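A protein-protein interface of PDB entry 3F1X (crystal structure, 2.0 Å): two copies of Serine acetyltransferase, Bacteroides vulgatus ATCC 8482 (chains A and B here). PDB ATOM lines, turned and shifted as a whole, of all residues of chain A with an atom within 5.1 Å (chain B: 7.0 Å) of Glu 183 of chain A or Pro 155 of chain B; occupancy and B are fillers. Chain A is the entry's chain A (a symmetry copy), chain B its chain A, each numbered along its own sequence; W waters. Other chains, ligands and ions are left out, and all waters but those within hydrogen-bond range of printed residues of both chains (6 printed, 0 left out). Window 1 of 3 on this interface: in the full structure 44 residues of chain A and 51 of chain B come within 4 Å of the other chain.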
ATOM      1  N   ARG A 179       9.301  35.296  24.296  1.00  0.00           N
ATOM      2  CA  ARG A 179       9.966  34.081  23.838  1.00  0.00           C
ATOM      3  C   ARG A 179       9.171  32.856  24.290  1.00  0.00           C
ATOM      4  O   ARG A 179       9.066  31.858  23.576  1.00  0.00           O
ATOM      5  CB  ARG A 179      11.394  34.029  24.390  1.00  0.00           C
ATOM      6  CG  ARG A 179      12.258  32.911  23.825  1.00  0.00           C
ATOM      7  CD  ARG A 179      12.357  32.980  22.305  1.00  0.00           C
ATOM      8  NE  ARG A 179      13.156  31.877  21.764  1.00  0.00           N
ATOM      9  CZ  ARG A 179      14.487  31.827  21.775  1.00  0.00           C
ATOM     10  NH1 ARG A 179      15.193  32.824  22.296  1.00  0.00           N
ATOM     11  NH2 ARG A 179      15.113  30.773  21.268  1.00  0.00           N
ATOM     12  N   PHE A 180       8.612  32.946  25.489  1.00  0.00           N
ATOM     13  CA  PHE A 180       7.795  31.882  26.044  1.00  0.00           C
ATOM     14  C   PHE A 180       6.648  31.615  25.091  1.00  0.00           C
ATOM     15  O   PHE A 180       6.358  30.470  24.742  1.00  0.00           O
ATOM     16  CB  PHE A 180       7.220  32.324  27.379  1.00  0.00           C
ATOM     17  CG  PHE A 180       7.646  31.485  28.524  1.00  0.00           C
ATOM     18  CD1 PHE A 180       6.985  30.293  28.813  1.00  0.00           C
ATOM     19  CD2 PHE A 180       8.712  31.882  29.328  1.00  0.00           C
ATOM     20  CE1 PHE A 180       7.375  29.507  29.889  1.00  0.00           C
ATOM     21  CE2 PHE A 180       9.112  31.100  30.409  1.00  0.00           C
ATOM     22  CZ  PHE A 180       8.441  29.907  30.692  1.00  0.00           C
ATOM     23  N   ILE A 181       5.992  32.688  24.673  1.00  0.00           N
ATOM     24  CA  ILE A 181       4.866  32.580  23.771  1.00  0.00           C
ATOM     25  C   ILE A 181       5.219  32.017  22.394  1.00  0.00           C
ATOM     26  O   ILE A 181       4.467  31.191  21.866  1.00  0.00           O
ATOM     27  CB  ILE A 181       4.147  33.952  23.648  1.00  0.00           C
ATOM     28  CG1 ILE A 181       3.457  34.259  24.990  1.00  0.00           C
ATOM     29  CG2 ILE A 181       3.165  33.947  22.466  1.00  0.00           C
ATOM     30  CD1 ILE A 181       2.676  35.561  25.042  1.00  0.00           C
ATOM     31  N   THR A 182       6.344  32.429  21.803  1.00  0.00           N
ATOM     32  CA  THR A 182       6.686  31.885  20.489  1.00  0.00           C
ATOM     33  C   THR A 182       7.126  30.430  20.570  1.00  0.00           C
ATOM     34  O   THR A 182       6.828  29.643  19.671  1.00  0.00           O
ATOM     35  CB  THR A 182       7.785  32.711  19.748  1.00  0.00           C
ATOM     36  OG1 THR A 182       8.961  32.832  20.564  1.00  0.00           O
ATOM     37  CG2 THR A 182       7.249  34.093  19.380  1.00  0.00           C
ATOM     38  N   GLU A 183       7.831  30.061  21.636  1.00  0.00           N
ATOM     39  CA  GLU A 183       8.258  28.672  21.782  1.00  0.00           C
ATOM     40  C   GLU A 183       7.033  27.791  21.972  1.00  0.00           C
ATOM     41  O   GLU A 183       7.055  26.603  21.649  1.00  0.00           O
ATOM     42  CB  GLU A 183       9.218  28.517  22.964  1.00  0.00           C
ATOM     43  CG  GLU A 183      10.580  29.146  22.710  1.00  0.00           C
ATOM     44  CD  GLU A 183      11.332  28.471  21.572  1.00  0.00           C
ATOM     45  OE1 GLU A 183      12.359  29.020  21.126  1.00  0.00           O
ATOM     46  OE2 GLU A 183      10.904  27.385  21.130  1.00  0.00           O
ATOM     47  N   MET A 184       5.963  28.382  22.500  1.00  0.00           N
ATOM     48  CA  MET A 184       4.717  27.653  22.705  1.00  0.00           C
ATOM     49  C   MET A 184       4.151  27.263  21.340  1.00  0.00           C
ATOM     50  O   MET A 184       3.685  26.135  21.144  1.00  0.00           O
ATOM     51  CB  MET A 184       3.714  28.533  23.457  1.00  0.00           C
ATOM     52  CG  MET A 184       3.172  27.912  24.727  1.00  0.00           C
ATOM     53  SD  MET A 184       1.928  29.099  25.617  1.00  0.00           S
ATOM     54  CE  MET A 184       0.418  28.871  24.425  1.00  0.00           C
ATOM     55  N   ALA A 185       4.186  28.206  20.402  1.00  0.00           N
ATOM     56  CA  ALA A 185       3.708  27.962  19.042  1.00  0.00           C
ATOM     57  C   ALA A 185       4.666  26.971  18.382  1.00  0.00           C
ATOM     58  O   ALA A 185       4.250  26.099  17.629  1.00  0.00           O
ATOM     59  CB  ALA A 185       3.682  29.266  18.244  1.00  0.00           C
ATOM     60  N   HIS A 186       5.951  27.128  18.679  1.00  0.00           N
ATOM     61  CA  HIS A 186       7.005  26.273  18.142  1.00  0.00           C
ATOM     62  C   HIS A 186       6.675  24.809  18.461  1.00  0.00           C
ATOM     63  O   HIS A 186       6.730  23.931  17.592  1.00  0.00           O
ATOM     64  CB  HIS A 186       8.338  26.686  18.781  1.00  0.00           C
ATOM     65  CG  HIS A 186       9.533  25.959  18.250  1.00  0.00           C
ATOM     66  ND1 HIS A 186       9.484  25.138  17.142  1.00  0.00           N
ATOM     67  CD2 HIS A 186      10.824  25.957  18.659  1.00  0.00           C
ATOM     68  CE1 HIS A 186      10.692  24.665  16.894  1.00  0.00           C
ATOM     69  NE2 HIS A 186      11.524  25.149  17.801  1.00  0.00           N
ATOM     70  N   SER A 187       6.301  24.565  19.712  1.00  0.00           N
ATOM     71  CA  SER A 187       5.954  23.228  20.175  1.00  0.00           C
ATOM     72  C   SER A 187       4.676  22.705  19.520  1.00  0.00           C
ATOM     73  O   SER A 187       4.640  21.567  19.070  1.00  0.00           O
ATOM     74  CB  SER A 187       5.769  23.232  21.701  1.00  0.00           C
ATOM     75  OG  SER A 187       5.315  21.967  22.162  1.00  0.00           O
ATOM     76  N   GLU A 188       3.644  23.545  19.462  1.00  0.00           N
ATOM     77  CA  GLU A 188       2.362  23.153  18.890  1.00  0.00           C
ATOM     78  C   GLU A 188       2.286  23.088  17.365  1.00  0.00           C
ATOM     79  O   GLU A 188       1.430  22.383  16.819  1.00  0.00           O
ATOM     80  CB  GLU A 188       1.245  24.086  19.383  1.00  0.00           C
ATOM     81  CG  GLU A 188       1.064  24.147  20.899  1.00  0.00           C
ATOM     82  CD  GLU A 188      -0.196  24.904  21.310  1.00  0.00           C
ATOM     83  OE1 GLU A 188      -1.307  24.442  20.961  1.00  0.00           O
ATOM     84  OE2 GLU A 188      -0.082  25.958  21.982  1.00  0.00           O
ATOM     85  N   ASP A 192       9.001  27.992  14.306  1.00  0.00           N
ATOM     86  CA  ASP A 192       9.775  28.777  15.268  1.00  0.00           C
ATOM     87  C   ASP A 192      10.116  30.181  14.765  1.00  0.00           C
ATOM     88  O   ASP A 192      10.994  30.361  13.915  1.00  0.00           O
ATOM     89  CB  ASP A 192      11.057  28.002  15.627  1.00  0.00           C
ATOM     90  CG  ASP A 192      11.872  28.662  16.736  1.00  0.00           C
ATOM     91  OD1 ASP A 192      11.278  29.245  17.664  1.00  0.00           O
ATOM     92  OD2 ASP A 192      13.121  28.577  16.688  1.00  0.00           O
ATOM     93  N   ILE B 150      16.483  29.570  29.288  1.00  0.00           N
ATOM     94  CA  ILE B 150      16.790  28.359  28.542  1.00  0.00           C
ATOM     95  C   ILE B 150      16.111  27.139  29.142  1.00  0.00           C
ATOM     96  O   ILE B 150      15.416  26.409  28.443  1.00  0.00           O
ATOM     97  CB  ILE B 150      18.309  28.135  28.479  1.00  0.00           C
ATOM     98  CG1 ILE B 150      18.939  29.245  27.625  1.00  0.00           C
ATOM     99  CG2 ILE B 150      18.616  26.757  27.910  1.00  0.00           C
ATOM    100  CD1 ILE B 150      20.442  29.196  27.555  1.00  0.00           C
ATOM    101  N   SER B 152      13.660  27.073  31.253  1.00  0.00           N
ATOM    102  CA  SER B 152      12.220  27.304  31.301  1.00  0.00           C
ATOM    103  C   SER B 152      11.392  27.128  30.031  1.00  0.00           C
ATOM    104  O   SER B 152      10.256  26.663  30.114  1.00  0.00           O
ATOM    105  CB  SER B 152      11.943  28.689  31.900  1.00  0.00           C
ATOM    106  OG  SER B 152      12.278  28.712  33.274  1.00  0.00           O
ATOM    107  N   CYS B 153      11.923  27.490  28.863  1.00  0.00           N
ATOM    108  CA  CYS B 153      11.125  27.339  27.653  1.00  0.00           C
ATOM    109  C   CYS B 153      11.810  26.843  26.386  1.00  0.00           C
ATOM    110  O   CYS B 153      11.141  26.623  25.377  1.00  0.00           O
ATOM    111  CB  CYS B 153      10.388  28.645  27.344  1.00  0.00           C
ATOM    112  SG  CYS B 153      11.428  30.007  26.777  1.00  0.00           S
ATOM    113  N   TYR B 154      13.127  26.675  26.410  1.00  0.00           N
ATOM    114  CA  TYR B 154      13.817  26.180  25.219  1.00  0.00           C
ATOM    115  C   TYR B 154      13.455  24.715  25.005  1.00  0.00           C
ATOM    116  O   TYR B 154      13.633  23.882  25.894  1.00  0.00           O
ATOM    117  CB  TYR B 154      15.326  26.323  25.376  1.00  0.00           C
ATOM    118  CG  TYR B 154      15.845  27.678  24.984  1.00  0.00           C
ATOM    119  CD1 TYR B 154      15.130  28.834  25.277  1.00  0.00           C
ATOM    120  CD2 TYR B 154      17.068  27.809  24.336  1.00  0.00           C
ATOM    121  CE1 TYR B 154      15.620  30.093  24.931  1.00  0.00           C
ATOM    122  CE2 TYR B 154      17.571  29.064  23.989  1.00  0.00           C
ATOM    123  CZ  TYR B 154      16.841  30.201  24.290  1.00  0.00           C
ATOM    124  OH  TYR B 154      17.332  31.443  23.953  1.00  0.00           O
ATOM    125  N   PRO B 155      12.933  24.382  23.817  1.00  0.00           N
ATOM    126  CA  PRO B 155      12.541  23.007  23.498  1.00  0.00           C
ATOM    127  C   PRO B 155      13.698  22.010  23.487  1.00  0.00           C
ATOM    128  O   PRO B 155      13.532  20.858  23.878  1.00  0.00           O
ATOM    129  CB  PRO B 155      11.882  23.150  22.130  1.00  0.00           C
ATOM    130  CG  PRO B 155      12.656  24.293  21.508  1.00  0.00           C
ATOM    131  CD  PRO B 155      12.749  25.271  22.655  1.00  0.00           C
ATOM    132  N   ALA B 156      14.868  22.460  23.049  1.00  0.00           N
ATOM    133  CA  ALA B 156      16.039  21.599  22.983  1.00  0.00           C
ATOM    134  C   ALA B 156      16.407  20.993  24.334  1.00  0.00           C
ATOM    135  O   ALA B 156      16.693  19.802  24.424  1.00  0.00           O
ATOM    136  CB  ALA B 156      17.221  22.370  22.419  1.00  0.00           C
ATOM    137  N   ILE B 157      16.403  21.808  25.385  1.00  0.00           N
ATOM    138  CA  ILE B 157      16.747  21.311  26.710  1.00  0.00           C
ATOM    139  C   ILE B 157      15.779  20.224  27.151  1.00  0.00           C
ATOM    140  O   ILE B 157      16.172  19.271  27.813  1.00  0.00           O
ATOM    141  CB  ILE B 157      16.739  22.434  27.763  1.00  0.00           C
ATOM    142  CG1 ILE B 157      17.782  23.482  27.396  1.00  0.00           C
ATOM    143  CG2 ILE B 157      17.072  21.861  29.144  1.00  0.00           C
ATOM    144  CD1 ILE B 157      19.205  22.959  27.409  1.00  0.00           C
ATOM    145  N   ARG B 158      14.515  20.372  26.769  1.00  0.00           N
ATOM    146  CA  ARG B 158      13.491  19.400  27.113  1.00  0.00           C
ATOM    147  C   ARG B 158      13.750  18.079  26.405  1.00  0.00           C
ATOM    148  O   ARG B 158      13.655  17.014  27.012  1.00  0.00           O
ATOM    149  CB  ARG B 158      12.105  19.942  26.742  1.00  0.00           C
ATOM    150  CG  ARG B 158      11.687  21.108  27.611  1.00  0.00           C
ATOM    151  CD  ARG B 158      10.393  21.761  27.155  1.00  0.00           C
ATOM    152  NE  ARG B 158      10.033  22.884  28.022  1.00  0.00           N
ATOM    153  CZ  ARG B 158       8.951  23.641  27.859  1.00  0.00           C
ATOM    154  NH1 ARG B 158       8.702  24.642  28.697  1.00  0.00           N
ATOM    155  NH2 ARG B 158       8.118  23.398  26.855  1.00  0.00           N
ATOM    156  N   ALA B 159      14.083  18.149  25.116  1.00  0.00           N
ATOM    157  CA  ALA B 159      14.363  16.941  24.341  1.00  0.00           C
ATOM    158  C   ALA B 159      15.624  16.258  24.864  1.00  0.00           C
ATOM    159  O   ALA B 159      15.646  15.046  25.057  1.00  0.00           O
ATOM    160  CB  ALA B 159      14.533  17.292  22.863  1.00  0.00           C
ATOM    161  N   ILE B 160      16.673  17.042  25.094  1.00  0.00           N
ATOM    162  CA  ILE B 160      17.933  16.497  25.590  1.00  0.00           C
ATOM    163  C   ILE B 160      17.744  15.903  26.989  1.00  0.00           C
ATOM    164  O   ILE B 160      18.315  14.862  27.315  1.00  0.00           O
ATOM    165  CB  ILE B 160      19.035  17.589  25.603  1.00  0.00           C
ATOM    166  CG1 ILE B 160      19.337  18.018  24.169  1.00  0.00           C
ATOM    167  CG2 ILE B 160      20.318  17.064  26.258  1.00  0.00           C
ATOM    168  CD1 ILE B 160      20.191  19.256  24.066  1.00  0.00           C
ATOM    169  N   SER B 161      16.934  16.559  27.813  1.00  0.00           N
ATOM    170  CA  SER B 161      16.662  16.054  29.154  1.00  0.00           C
ATOM    171  C   SER B 161      15.956  14.710  29.049  1.00  0.00           C
ATOM    172  O   SER B 161      16.357  13.744  29.699  1.00  0.00           O
ATOM    173  CB  SER B 161      15.780  17.032  29.930  1.00  0.00           C
ATOM    174  OG  SER B 161      16.462  18.243  30.168  1.00  0.00           O
ATOM    175  N   ALA B 185       9.203  13.427  23.704  1.00  0.00           N
ATOM    176  CA  ALA B 185       9.927  14.666  23.419  1.00  0.00           C
ATOM    177  C   ALA B 185       9.786  14.955  21.925  1.00  0.00           C
ATOM    178  O   ALA B 185       9.649  16.101  21.516  1.00  0.00           O
ATOM    179  CB  ALA B 185      11.405  14.513  23.779  1.00  0.00           C
ATOM    180  N   GLU B 188       6.496  16.650  21.424  1.00  0.00           N
ATOM    181  CA  GLU B 188       6.480  17.991  21.995  1.00  0.00           C
ATOM    182  C   GLU B 188       7.489  18.986  21.425  1.00  0.00           C
ATOM    183  O   GLU B 188       7.280  20.201  21.519  1.00  0.00           O
ATOM    184  CB  GLU B 188       6.681  17.930  23.517  1.00  0.00           C
ATOM    185  CG  GLU B 188       5.647  17.102  24.280  1.00  0.00           C
ATOM    186  CD  GLU B 188       5.763  17.267  25.793  1.00  0.00           C
ATOM    187  OE1 GLU B 188       5.561  18.402  26.283  1.00  0.00           O
ATOM    188  OE2 GLU B 188       6.055  16.268  26.495  1.00  0.00           O
ATOM    189  N   THR B 189       8.574  18.500  20.827  1.00  0.00           N
ATOM    190  CA  THR B 189       9.603  19.408  20.309  1.00  0.00           C
ATOM    191  C   THR B 189      10.009  19.240  18.850  1.00  0.00           C
ATOM    192  O   THR B 189      10.672  20.111  18.292  1.00  0.00           O
ATOM    193  CB  THR B 189      10.903  19.285  21.129  1.00  0.00           C
ATOM    194  OG1 THR B 189      11.478  17.989  20.901  1.00  0.00           O
ATOM    195  CG2 THR B 189      10.617  19.459  22.620  1.00  0.00           C
ATOM    196  N   GLY B 190       9.632  18.123  18.242  1.00  0.00           N
ATOM    197  CA  GLY B 190      10.004  17.873  16.865  1.00  0.00           C
ATOM    198  C   GLY B 190      11.418  17.310  16.777  1.00  0.00           C
ATOM    199  O   GLY B 190      11.942  17.099  15.677  1.00  0.00           O
ATOM    200  N   ILE B 191      12.027  17.057  17.935  1.00  0.00           N
ATOM    201  CA  ILE B 191      13.384  16.514  18.038  1.00  0.00           C
ATOM    202  C   ILE B 191      13.310  15.026  18.393  1.00  0.00           C
ATOM    203  O   ILE B 191      12.816  14.663  19.460  1.00  0.00           O
ATOM    204  CB  ILE B 191      14.196  17.263  19.135  1.00  0.00           C
ATOM    205  CG1 ILE B 191      14.210  18.755  18.840  1.00  0.00           C
ATOM    206  CG2 ILE B 191      15.635  16.744  19.170  1.00  0.00           C
ATOM    207  CD1 ILE B 191      14.762  19.612  19.955  1.00  0.00           C
ATOM    208  N   ILE B 205      21.304  21.784  20.677  1.00  0.00           N
ATOM    209  CA  ILE B 205      20.520  21.687  19.458  1.00  0.00           C
ATOM    210  C   ILE B 205      19.843  23.040  19.313  1.00  0.00           C
ATOM    211  O   ILE B 205      19.086  23.456  20.189  1.00  0.00           O
ATOM    212  CB  ILE B 205      19.447  20.581  19.563  1.00  0.00           C
ATOM    213  CG1 ILE B 205      20.128  19.207  19.623  1.00  0.00           C
ATOM    214  CG2 ILE B 205      18.496  20.673  18.379  1.00  0.00           C
ATOM    215  CD1 ILE B 205      19.183  18.041  19.880  1.00  0.00           C
ATOM    216  N   HIS B 207      17.154  25.403  17.823  1.00  0.00           N
ATOM    217  CA  HIS B 207      15.833  25.348  17.198  1.00  0.00           C
ATOM    218  C   HIS B 207      15.397  23.873  17.200  1.00  0.00           C
ATOM    219  O   HIS B 207      14.454  23.507  17.903  1.00  0.00           O
ATOM    220  CB  HIS B 207      15.921  25.944  15.790  1.00  0.00           C
ATOM    221  CG  HIS B 207      16.617  27.274  15.750  1.00  0.00           C
ATOM    222  ND1 HIS B 207      16.140  28.383  16.419  1.00  0.00           N
ATOM    223  CD2 HIS B 207      17.751  27.671  15.128  1.00  0.00           C
ATOM    224  CE1 HIS B 207      16.948  29.408  16.203  1.00  0.00           C
ATOM    225  NE2 HIS B 207      17.933  29.006  15.423  1.00  0.00           N
ATOM    226  N   GLY B 208      16.074  23.046  16.408  1.00  0.00           N
ATOM    227  CA  GLY B 208      15.829  21.614  16.434  1.00  0.00           C
ATOM    228  C   GLY B 208      14.707  20.839  15.769  1.00  0.00           C
ATOM    229  O   GLY B 208      14.821  19.619  15.673  1.00  0.00           O
ATOM    230  N   THR B 209      13.635  21.485  15.328  1.00  0.00           N
ATOM    231  CA  THR B 209      12.545  20.736  14.690  1.00  0.00           C
ATOM    232  C   THR B 209      13.067  19.934  13.499  1.00  0.00           C
ATOM    233  O   THR B 209      13.746  20.469  12.629  1.00  0.00           O
ATOM    234  CB  THR B 209      11.425  21.684  14.232  1.00  0.00           C
ATOM    235  OG1 THR B 209      10.871  22.326  15.383  1.00  0.00           O
ATOM    236  CG2 THR B 209      10.313  20.923  13.525  1.00  0.00           C
HETATM  237  O   HOH W   1       6.995  20.094  17.813  1.00  0.00           O
HETATM  238  O   HOH W   2      13.084  24.512  15.004  1.00  0.00           O
HETATM  239  O   HOH W   3       9.557  23.085  19.510  1.00  0.00           O
HETATM  240  O   HOH W   4      17.605  31.766  21.203  1.00  0.00           O
HETATM  241  O   HOH W   5      12.411  22.206  19.055  1.00  0.00           O
HETATM  242  O   HOH W   6       8.867  21.691  16.876  1.00  0.00           O
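OH of Tyr 154 of chain B sits at hydrogen-bond distance from NH1 of Arg 179 of chain A (3.0 Å).
The side-chain hydroxyl (OG) of Ser 187 of chain A is in hydrogen-bond range of the backbone carbonyl oxygen (O) of Glu 188 of chain B (2.7 Å).
The backbone carbonyl oxygen (O) of His 207 of chain B is in hydrogen-bond range of a ring nitrogen (NE2) of His 186 of chain A (3.4 Å).
The side-chain carboxylate (OD2) of Asp 192 of chain A sits at hydrogen-bond distance from a ring nitrogen (ND1) of His 207 of chain B, at 3.0 Å.
The backbone carbonyl oxygen (O) of Ser 152 of chain B sits at hydrogen-bond distance from the guanidinium group (NH1) of Arg 158 of chain B, at 2.9 Å.
The backbone carbonyl oxygen (O) of Arg 179 of chain A is in hydrogen-bond range of the side-chain hydroxyl (OG1) of Thr 182 of chain A, 3.2 Å away.
NE of Arg 179 of chain A lies within salt-bridge range of OE1 of Glu 183 of chain A (3.0 Å).
Among the printed residues, merely in contact across the chains: Phe 180 of chain A with Ser 152 of chain B, Glu 183 of chain A with Cys 153 of chain B, Glu 183 of chain A with Pro 155 of chain B, His 186 of chain A with Pro 155 of chain B and His 186 of chain A with Thr 209 of chain B.
Glu 183 of chain A touches two residues of chain B.
Of the printed residues of chain B, His 186 of chain A touches Pro 155 (3.8 Å), His 207 (3.4 Å) and Thr 209 (2.8 Å).
Printed residues of chain B within 4 Å of Ser 187 of chain A: Glu 188 (2.7 Å).
Printed residues of chain A within 4 Å of Cys 153 of chain B: Glu 183 (3.6 Å).
Of the printed residues of chain A, Tyr 154 of chain B touches Arg 179.
Pro 155 of chain B touches just these residues of chain A: Glu 183 (3.2 Å) and His 186 (3.8 Å).
Ala 159 of chain B touches none of the printed residues of chain A.
Thr 189 of chain B touches none of the printed residues of chain A.
Printed residues of chain A within 4 Å of His 207 of chain B: His 186 and Asp 192.
The nearest residue of chain B that does not touch Glu 183 of chain A is Tyr 154 of chain B (5.0 Å).
The nearest printed residue of chain A that does not touch Thr 209 of chain B is Asp 192 of chain A (5.7 Å).
Along chain A the printed residues that touch a printed residue of chain B span positions 179 to 192.
Of the 20 printed residues of chain B, 7 touch a printed residue of chain A.
Printed residues of chain B that touch a printed residue of chain A: Ser 152, Cys 153, Tyr 154, Pro 155, Glu 188, His 207 and Thr 209.
Hydrophobic or aromatic side chains of chain B within 4 Å of the printed part of chain A: Tyr 154, Pro 155 and His 207.
Among the printed residues, 9 pairs touch across the chains.
Positions printed for both chains: 185 and 188.
Water W6 lies within hydrogen-bond range of the side-chain hydroxyl of Thr 209 of chain B (2.6 Å), the backbone carbonyl oxygen of Thr 189 of chain B (2.8 Å) and the backbone carbonyl oxygen of His 186 of chain A (3.2 Å).
Water W5 lies within hydrogen-bond range of the backbone carbonyl oxygen (O) of His 207 of chain B (2.7 Å), the backbone carbonyl oxygen (O) of Thr 189 of chain B (2.8 Å) and a ring nitrogen (NE2) of His 186 of chain A (3.3 Å).
Water W4 lies within hydrogen-bond range of NH2 of Arg 179 of chain A (2.7 Å) and OH of Tyr 154 of chain B (2.8 Å).
Water W1 lies within hydrogen-bond range of the backbone carbonyl oxygen (O) of Ser 187 of chain A (3.0 Å) and the backbone NH (N) of Gly 190 of chain B (3.3 Å).
Water W2 lies within hydrogen-bond range of the backbone NH (N) of Thr 209 of chain B (3.1 Å), a ring nitrogen (NE2) of His 186 of chain A (3.3 Å) and the backbone carbonyl oxygen (O) of His 207 of chain B (3.4 Å).
Water W3 bridges a ring nitrogen (ND1) of His 186 of chain A (3.1 Å) and the backbone carbonyl oxygen (O) of Thr 189 of chain B (3.4 Å).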
